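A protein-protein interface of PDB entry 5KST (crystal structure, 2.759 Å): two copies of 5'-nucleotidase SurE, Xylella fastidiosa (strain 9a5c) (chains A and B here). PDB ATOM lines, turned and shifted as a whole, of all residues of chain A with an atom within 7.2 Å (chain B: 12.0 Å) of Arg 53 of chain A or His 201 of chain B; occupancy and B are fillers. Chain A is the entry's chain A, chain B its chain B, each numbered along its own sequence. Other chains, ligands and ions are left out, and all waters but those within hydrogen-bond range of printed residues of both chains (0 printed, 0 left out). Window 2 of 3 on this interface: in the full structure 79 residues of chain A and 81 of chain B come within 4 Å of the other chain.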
ATOM      1  N   ASP A  36      -2.814   0.086  18.876  1.00  0.00           N
ATOM      2  CA  ASP A  36      -1.809   0.449  17.889  1.00  0.00           C
ATOM      3  C   ASP A  36      -0.697   1.252  18.551  1.00  0.00           C
ATOM      4  O   ASP A  36       0.470   1.131  18.191  1.00  0.00           O
ATOM      5  CB  ASP A  36      -2.441   1.234  16.732  1.00  0.00           C
ATOM      6  CG  ASP A  36      -3.204   2.471  17.198  1.00  0.00           C
ATOM      7  OD1 ASP A  36      -3.693   2.497  18.351  1.00  0.00           O
ATOM      8  OD2 ASP A  36      -3.322   3.429  16.400  1.00  0.00           O
ATOM      9  N   PRO A  51     -16.282   4.060  15.383  1.00  0.00           N
ATOM     10  CA  PRO A  51     -15.883   2.702  15.056  1.00  0.00           C
ATOM     11  C   PRO A  51     -14.413   2.535  15.330  1.00  0.00           C
ATOM     12  O   PRO A  51     -13.703   3.526  15.500  1.00  0.00           O
ATOM     13  CB  PRO A  51     -16.169   2.605  13.562  1.00  0.00           C
ATOM     14  CG  PRO A  51     -15.883   3.966  13.075  1.00  0.00           C
ATOM     15  CD  PRO A  51     -16.346   4.889  14.175  1.00  0.00           C
ATOM     16  N   ILE A  52     -13.961   1.293  15.355  1.00  0.00           N
ATOM     17  CA  ILE A  52     -12.588   0.998  15.692  1.00  0.00           C
ATOM     18  C   ILE A  52     -11.927   0.281  14.528  1.00  0.00           C
ATOM     19  O   ILE A  52     -12.509  -0.621  13.942  1.00  0.00           O
ATOM     20  CB  ILE A  52     -12.513   0.151  16.961  1.00  0.00           C
ATOM     21  CG1 ILE A  52     -13.312   0.827  18.077  1.00  0.00           C
ATOM     22  CG2 ILE A  52     -11.083  -0.017  17.386  1.00  0.00           C
ATOM     23  CD1 ILE A  52     -13.823  -0.124  19.137  1.00  0.00           C
ATOM     24  N   ARG A  53     -10.721   0.705  14.177  1.00  0.00           N
ATOM     25  CA  ARG A  53      -9.981   0.056  13.113  1.00  0.00           C
ATOM     26  C   ARG A  53      -9.065  -1.005  13.687  1.00  0.00           C
ATOM     27  O   ARG A  53      -8.378  -0.773  14.670  1.00  0.00           O
ATOM     28  CB  ARG A  53      -9.166   1.072  12.327  1.00  0.00           C
ATOM     29  CG  ARG A  53      -9.968   2.208  11.776  1.00  0.00           C
ATOM     30  CD  ARG A  53      -9.355   2.613  10.459  1.00  0.00           C
ATOM     31  NE  ARG A  53     -10.122   3.649   9.846  1.00  0.00           N
ATOM     32  CZ  ARG A  53     -10.825   3.679   8.718  1.00  0.00           C
ATOM     33  NH1 ARG A  53     -11.431   4.823   8.484  1.00  0.00           N
ATOM     34  NH2 ARG A  53     -10.937   2.686   7.839  1.00  0.00           N
ATOM     35  N   ALA A  54      -9.059  -2.179  13.071  1.00  0.00           N
ATOM     36  CA  ALA A  54      -8.154  -3.239  13.494  1.00  0.00           C
ATOM     37  C   ALA A  54      -7.296  -3.670  12.324  1.00  0.00           C
ATOM     38  O   ALA A  54      -7.809  -4.116  11.298  1.00  0.00           O
ATOM     39  CB  ALA A  54      -8.925  -4.422  14.061  1.00  0.00           C
ATOM     40  N   LYS A  55      -5.988  -3.513  12.478  1.00  0.00           N
ATOM     41  CA  LYS A  55      -5.040  -3.934  11.457  1.00  0.00           C
ATOM     42  C   LYS A  55      -4.444  -5.264  11.874  1.00  0.00           C
ATOM     43  O   LYS A  55      -3.991  -5.412  13.006  1.00  0.00           O
ATOM     44  CB  LYS A  55      -3.945  -2.876  11.261  1.00  0.00           C
ATOM     45  CG  LYS A  55      -2.883  -3.239  10.235  1.00  0.00           C
ATOM     46  N   SER A  63      -3.407  -5.139  15.415  1.00  0.00           N
ATOM     47  CA  SER A  63      -3.178  -3.794  15.914  1.00  0.00           C
ATOM     48  C   SER A  63      -4.487  -3.037  15.889  1.00  0.00           C
ATOM     49  O   SER A  63      -5.073  -2.843  14.828  1.00  0.00           O
ATOM     50  CB  SER A  63      -2.130  -3.071  15.077  1.00  0.00           C
ATOM     51  OG  SER A  63      -1.864  -1.784  15.603  1.00  0.00           O
ATOM     52  N   VAL A  64      -4.943  -2.611  17.062  1.00  0.00           N
ATOM     53  CA  VAL A  64      -6.253  -1.991  17.195  1.00  0.00           C
ATOM     54  C   VAL A  64      -6.169  -0.524  17.595  1.00  0.00           C
ATOM     55  O   VAL A  64      -5.630  -0.191  18.646  1.00  0.00           O
ATOM     56  CB  VAL A  64      -7.105  -2.737  18.232  1.00  0.00           C
ATOM     57  CG1 VAL A  64      -8.450  -2.056  18.397  1.00  0.00           C
ATOM     58  CG2 VAL A  64      -7.281  -4.185  17.821  1.00  0.00           C
ATOM     59  N   ALA A  65      -6.717   0.346  16.753  1.00  0.00           N
ATOM     60  CA  ALA A  65      -6.752   1.774  17.036  1.00  0.00           C
ATOM     61  C   ALA A  65      -7.865   2.094  18.026  1.00  0.00           C
ATOM     62  O   ALA A  65      -8.862   2.729  17.677  1.00  0.00           O
ATOM     63  CB  ALA A  65      -6.935   2.564  15.756  1.00  0.00           C
ATOM     64  N   GLY A  66      -7.683   1.650  19.265  1.00  0.00           N
ATOM     65  CA  GLY A  66      -8.680   1.824  20.306  1.00  0.00           C
ATOM     66  C   GLY A  66      -8.150   1.372  21.651  1.00  0.00           C
ATOM     67  O   GLY A  66      -6.985   0.997  21.776  1.00  0.00           O
ATOM     68  N   LEU A  74     -13.551  -6.410  21.032  1.00  0.00           N
ATOM     69  CA  LEU A  74     -13.556  -6.761  19.615  1.00  0.00           C
ATOM     70  C   LEU A  74     -13.105  -8.201  19.403  1.00  0.00           C
ATOM     71  O   LEU A  74     -13.761  -8.965  18.693  1.00  0.00           O
ATOM     72  CB  LEU A  74     -12.658  -5.816  18.815  1.00  0.00           C
ATOM     73  CG  LEU A  74     -13.173  -4.390  18.653  1.00  0.00           C
ATOM     74  CD1 LEU A  74     -12.260  -3.608  17.724  1.00  0.00           C
ATOM     75  CD2 LEU A  74     -14.623  -4.380  18.158  1.00  0.00           C
ATOM     76  N   LEU A  79     -14.243 -10.062  16.009  1.00  0.00           N
ATOM     77  CA  LEU A  79     -13.070  -9.696  15.231  1.00  0.00           C
ATOM     78  C   LEU A  79     -12.332 -10.961  14.809  1.00  0.00           C
ATOM     79  O   LEU A  79     -11.798 -11.050  13.701  1.00  0.00           O
ATOM     80  CB  LEU A  79     -12.132  -8.786  16.022  1.00  0.00           C
ATOM     81  CG  LEU A  79     -10.843  -8.405  15.284  1.00  0.00           C
ATOM     82  CD1 LEU A  79     -11.155  -7.456  14.138  1.00  0.00           C
ATOM     83  CD2 LEU A  79      -9.818  -7.797  16.230  1.00  0.00           C
ATOM     84  N   CYS B 192     -19.743  -7.271  18.072  1.00  0.00           N
ATOM     85  CA  CYS B 192     -18.885  -6.456  17.227  1.00  0.00           C
ATOM     86  C   CYS B 192     -19.473  -6.376  15.829  1.00  0.00           C
ATOM     87  O   CYS B 192     -19.639  -7.392  15.158  1.00  0.00           O
ATOM     88  CB  CYS B 192     -17.467  -7.028  17.188  1.00  0.00           C
ATOM     89  SG  CYS B 192     -16.502  -6.560  15.743  1.00  0.00           S
ATOM     90  N   LEU B 193     -19.796  -5.164  15.395  1.00  0.00           N
ATOM     91  CA  LEU B 193     -20.404  -4.965  14.085  1.00  0.00           C
ATOM     92  C   LEU B 193     -19.362  -4.531  13.061  1.00  0.00           C
ATOM     93  O   LEU B 193     -18.727  -3.490  13.201  1.00  0.00           O
ATOM     94  CB  LEU B 193     -21.542  -3.944  14.178  1.00  0.00           C
ATOM     95  CG  LEU B 193     -22.602  -4.331  15.216  1.00  0.00           C
ATOM     96  CD1 LEU B 193     -23.730  -3.314  15.290  1.00  0.00           C
ATOM     97  CD2 LEU B 193     -23.153  -5.724  14.926  1.00  0.00           C
ATOM     98  N   THR B 194     -19.190  -5.350  12.032  1.00  0.00           N
ATOM     99  CA  THR B 194     -18.174  -5.117  11.015  1.00  0.00           C
ATOM    100  C   THR B 194     -18.745  -4.352   9.823  1.00  0.00           C
ATOM    101  O   THR B 194     -19.353  -4.944   8.933  1.00  0.00           O
ATOM    102  CB  THR B 194     -17.566  -6.452  10.528  1.00  0.00           C
ATOM    103  OG1 THR B 194     -16.977  -7.142  11.636  1.00  0.00           O
ATOM    104  CG2 THR B 194     -16.503  -6.214   9.475  1.00  0.00           C
ATOM    105  N   GLN B 195     -18.554  -3.035   9.820  1.00  0.00           N
ATOM    106  CA  GLN B 195     -18.984  -2.192   8.708  1.00  0.00           C
ATOM    107  C   GLN B 195     -17.778  -1.666   7.944  1.00  0.00           C
ATOM    108  O   GLN B 195     -16.639  -2.024   8.247  1.00  0.00           O
ATOM    109  CB  GLN B 195     -19.842  -1.032   9.205  1.00  0.00           C
ATOM    110  CG  GLN B 195     -21.078  -1.468   9.968  1.00  0.00           C
ATOM    111  CD  GLN B 195     -21.944  -0.297  10.402  1.00  0.00           C
ATOM    112  OE1 GLN B 195     -21.470   0.838  10.517  1.00  0.00           O
ATOM    113  NE2 GLN B 195     -23.224  -0.566  10.637  1.00  0.00           N
ATOM    114  N   THR B 196     -18.026  -0.826   6.943  1.00  0.00           N
ATOM    115  CA  THR B 196     -16.944  -0.279   6.130  1.00  0.00           C
ATOM    116  C   THR B 196     -17.064   1.229   5.977  1.00  0.00           C
ATOM    117  O   THR B 196     -18.148   1.753   5.743  1.00  0.00           O
ATOM    118  CB  THR B 196     -16.906  -0.907   4.734  1.00  0.00           C
ATOM    119  OG1 THR B 196     -18.102  -0.561   4.033  1.00  0.00           O
ATOM    120  CG2 THR B 196     -16.787  -2.424   4.824  1.00  0.00           C
ATOM    121  N   ASP B 197     -15.938   1.921   6.105  1.00  0.00           N
ATOM    122  CA  ASP B 197     -15.905   3.369   5.960  1.00  0.00           C
ATOM    123  C   ASP B 197     -16.129   3.745   4.492  1.00  0.00           C
ATOM    124  O   ASP B 197     -16.145   2.864   3.628  1.00  0.00           O
ATOM    125  CB  ASP B 197     -14.574   3.920   6.505  1.00  0.00           C
ATOM    126  CG  ASP B 197     -13.393   3.660   5.584  1.00  0.00           C
ATOM    127  OD1 ASP B 197     -13.490   2.808   4.677  1.00  0.00           O
ATOM    128  OD2 ASP B 197     -12.345   4.313   5.788  1.00  0.00           O
ATOM    129  N   PRO B 198     -16.337   5.043   4.207  1.00  0.00           N
ATOM    130  CA  PRO B 198     -16.480   5.542   2.832  1.00  0.00           C
ATOM    131  C   PRO B 198     -15.408   5.052   1.866  1.00  0.00           C
ATOM    132  O   PRO B 198     -15.700   4.841   0.690  1.00  0.00           O
ATOM    133  CB  PRO B 198     -16.374   7.064   3.002  1.00  0.00           C
ATOM    134  CG  PRO B 198     -16.208   7.316   4.496  1.00  0.00           C
ATOM    135  CD  PRO B 198     -16.693   6.089   5.176  1.00  0.00           C
ATOM    136  N   ARG B 199     -14.184   4.882   2.355  1.00  0.00           N
ATOM    137  CA  ARG B 199     -13.087   4.405   1.522  1.00  0.00           C
ATOM    138  C   ARG B 199     -13.258   2.930   1.169  1.00  0.00           C
ATOM    139  O   ARG B 199     -12.641   2.428   0.226  1.00  0.00           O
ATOM    140  CB  ARG B 199     -11.752   4.628   2.230  1.00  0.00           C
ATOM    141  CG  ARG B 199     -11.444   6.086   2.514  1.00  0.00           C
ATOM    142  CD  ARG B 199     -10.440   6.214   3.642  1.00  0.00           C
ATOM    143  NE  ARG B 199      -9.992   7.590   3.830  1.00  0.00           N
ATOM    144  CZ  ARG B 199      -9.210   7.988   4.829  1.00  0.00           C
ATOM    145  NH1 ARG B 199      -8.795   7.114   5.739  1.00  0.00           N
ATOM    146  NH2 ARG B 199      -8.847   9.258   4.921  1.00  0.00           N
ATOM    147  N   GLY B 200     -14.108   2.243   1.925  1.00  0.00           N
ATOM    148  CA  GLY B 200     -14.338   0.824   1.729  1.00  0.00           C
ATOM    149  C   GLY B 200     -13.603  -0.011   2.759  1.00  0.00           C
ATOM    150  O   GLY B 200     -13.849  -1.210   2.890  1.00  0.00           O
ATOM    151  N   HIS B 201     -12.697   0.631   3.493  1.00  0.00           N
ATOM    152  CA  HIS B 201     -11.909  -0.053   4.511  1.00  0.00           C
ATOM    153  C   HIS B 201     -12.765  -0.484   5.690  1.00  0.00           C
ATOM    154  O   HIS B 201     -13.632   0.256   6.151  1.00  0.00           O
ATOM    155  CB  HIS B 201     -10.762   0.833   4.989  1.00  0.00           C
ATOM    156  CG  HIS B 201      -9.624   0.902   4.023  1.00  0.00           C
ATOM    157  ND1 HIS B 201      -8.880  -0.207   3.677  1.00  0.00           N
ATOM    158  CD2 HIS B 201      -9.110   1.937   3.322  1.00  0.00           C
ATOM    159  CE1 HIS B 201      -7.955   0.145   2.802  1.00  0.00           C
ATOM    160  NE2 HIS B 201      -8.070   1.440   2.569  1.00  0.00           N
ATOM    161  N   THR B 202     -12.513  -1.694   6.170  1.00  0.00           N
ATOM    162  CA  THR B 202     -13.344  -2.289   7.199  1.00  0.00           C
ATOM    163  C   THR B 202     -13.102  -1.648   8.557  1.00  0.00           C
ATOM    164  O   THR B 202     -11.967  -1.537   9.019  1.00  0.00           O
ATOM    165  CB  THR B 202     -13.111  -3.806   7.290  1.00  0.00           C
ATOM    166  OG1 THR B 202     -13.779  -4.457   6.199  1.00  0.00           O
ATOM    167  CG2 THR B 202     -13.651  -4.349   8.598  1.00  0.00           C
ATOM    168  N   ILE B 203     -14.189  -1.209   9.179  1.00  0.00           N
ATOM    169  CA  ILE B 203     -14.155  -0.671  10.527  1.00  0.00           C
ATOM    170  C   ILE B 203     -15.040  -1.523  11.424  1.00  0.00           C
ATOM    171  O   ILE B 203     -15.908  -2.248  10.941  1.00  0.00           O
ATOM    172  CB  ILE B 203     -14.640   0.775  10.567  1.00  0.00           C
ATOM    173  CG1 ILE B 203     -15.988   0.874   9.851  1.00  0.00           C
ATOM    174  CG2 ILE B 203     -13.611   1.698   9.932  1.00  0.00           C
ATOM    175  CD1 ILE B 203     -16.644   2.197   9.995  1.00  0.00           C
ATOM    176  N   TYR B 204     -14.830  -1.430  12.729  1.00  0.00           N
ATOM    177  CA  TYR B 204     -15.577  -2.269  13.653  1.00  0.00           C
ATOM    178  C   TYR B 204     -16.276  -1.426  14.698  1.00  0.00           C
ATOM    179  O   TYR B 204     -15.629  -0.791  15.526  1.00  0.00           O
ATOM    180  CB  TYR B 204     -14.652  -3.295  14.326  1.00  0.00           C
ATOM    181  CG  TYR B 204     -13.868  -4.151  13.350  1.00  0.00           C
ATOM    182  CD1 TYR B 204     -14.384  -5.346  12.873  1.00  0.00           C
ATOM    183  CD2 TYR B 204     -12.610  -3.756  12.902  1.00  0.00           C
ATOM    184  CE1 TYR B 204     -13.671  -6.128  11.981  1.00  0.00           C
ATOM    185  CE2 TYR B 204     -11.890  -4.530  12.013  1.00  0.00           C
ATOM    186  CZ  TYR B 204     -12.424  -5.714  11.553  1.00  0.00           C
ATOM    187  OH  TYR B 204     -11.710  -6.492  10.663  1.00  0.00           O
ATOM    188  N   TRP B 205     -17.600  -1.414  14.654  1.00  0.00           N
ATOM    189  CA  TRP B 205     -18.371  -0.785  15.713  1.00  0.00           C
ATOM    190  C   TRP B 205     -18.606  -1.777  16.836  1.00  0.00           C
ATOM    191  O   TRP B 205     -18.818  -2.962  16.585  1.00  0.00           O
ATOM    192  CB  TRP B 205     -19.721  -0.279  15.201  1.00  0.00           C
ATOM    193  CG  TRP B 205     -19.660   0.887  14.270  1.00  0.00           C
ATOM    194  CD1 TRP B 205     -19.559   0.849  12.907  1.00  0.00           C
ATOM    195  CD2 TRP B 205     -19.732   2.267  14.628  1.00  0.00           C
ATOM    196  NE1 TRP B 205     -19.547   2.124  12.397  1.00  0.00           N
ATOM    197  CE2 TRP B 205     -19.655   3.014  13.434  1.00  0.00           C
ATOM    198  CE3 TRP B 205     -19.850   2.946  15.843  1.00  0.00           C
ATOM    199  CZ2 TRP B 205     -19.690   4.406  13.420  1.00  0.00           C
ATOM    200  CZ3 TRP B 205     -19.883   4.327  15.827  1.00  0.00           C
ATOM    201  CH2 TRP B 205     -19.804   5.043  14.622  1.00  0.00           C
ATOM    202  N   ILE B 206     -18.568  -1.301  18.074  1.00  0.00           N
ATOM    203  CA  ILE B 206     -19.133  -2.077  19.161  1.00  0.00           C
ATOM    204  C   ILE B 206     -20.640  -1.874  19.123  1.00  0.00           C
ATOM    205  O   ILE B 206     -21.132  -0.762  19.327  1.00  0.00           O
ATOM    206  CB  ILE B 206     -18.573  -1.674  20.520  1.00  0.00           C
ATOM    207  CG1 ILE B 206     -17.083  -2.023  20.592  1.00  0.00           C
ATOM    208  CG2 ILE B 206     -19.347  -2.373  21.632  1.00  0.00           C
ATOM    209  CD1 ILE B 206     -16.429  -1.644  21.899  1.00  0.00           C
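Of the printed residues of chain B, Pro 51 of chain A touches Ile 203 (3.6 Å), Tyr 204 (3.5 Å) and Trp 205 (3.5 Å). Of chain B, only Asp 197, His 201 and Ile 203 come within 4 Å of Arg 53 of chain A. Of the printed residues of chain B, Ala 54 of chain A touches Tyr 204. No residue of chain B comes within 4 Å of Val 64 of chain A. Of the printed residues of chain A, Cys 192 of chain B touches Leu 74 (3.8 Å). Gln 195 of chain B touches none of the printed residues of chain A. His 201 of chain B touches just one residue of chain A: Arg 53 (3.4 Å). Of the printed residues of chain A, Ile 203 of chain B touches Pro 51, Ile 52 and Arg 53. The nearest residue of chain B that does not touch Arg 53 of chain A is Arg 199 of chain B (4.4 Å). The nearest printed residue of chain A that does not touch His 201 of chain B is Ile 52 of chain A (7.9 Å). The nearest printed residue of chain A that does not touch Cys 192 of chain B is Leu 79 of chain A (4.2 Å).
No position is printed for both chains.
N of Ile 52 of chain A sits at hydrogen-bond distance from O of Tyr 204 of chain B. The side-chain carboxylate of Asp 197 of chain B is in salt-bridge range of the guanidinium group of Arg 53 of chain A.
Along chain B the printed residues that touch a printed residue of chain A span positions 192 to 205. Of the 12 printed residues of chain A, 6 touch a printed residue of chain B. Among the printed residues, 12 pairs touch across the chains. Among the printed residues, Asp or Glu carboxylates within 4 Å of a Lys or Arg side-chain nitrogen of the other chain: Arg 53 of chain A with Asp 197 of chain B (2.9 Å).
The backbone NH (N) of Leu 193 of chain B sits at hydrogen-bond distance from the backbone carbonyl oxygen (O) of Trp 205 of chain B. NE1 of Trp 205 of chain B sits at hydrogen-bond distance from OE1 of Gln 195 of chain B, at 3.0 Å. The side-chain carboxylate of Asp 197 of chain B lies close to the backbone NH of Arg 199 of chain B, at 3.2 Å. OD1 of Asp 197 of chain B is in hydrogen-bond range of N of Gly 200 of chain B (2.9 Å). The side-chain carboxylate of Asp 197 of chain B lies within hydrogen-bond range of the backbone NH of His 201 of chain B, at 2.6 Å. O of Arg 53 of chain A is in hydrogen-bond range of N of Ala 65 of chain A.
Among the printed residues, merely in contact across the chains: Pro 51 of chain A with Ile 203 of chain B, Pro 51 of chain A with Tyr 204 of chain B, Pro 51 of chain A with Trp 205 of chain B, Ile 52 of chain A with Ile 203 of chain B, Arg 53 of chain A with His 201 of chain B, Arg 53 of chain A with Ile 203 of chain B, Ala 54 of chain A with Tyr 204 of chain B, Leu 74 of chain A with Cys 192 of chain B, Leu 74 of chain A with Tyr 204 of chain B and Leu 79 of chain A with Tyr 204 of chain B.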
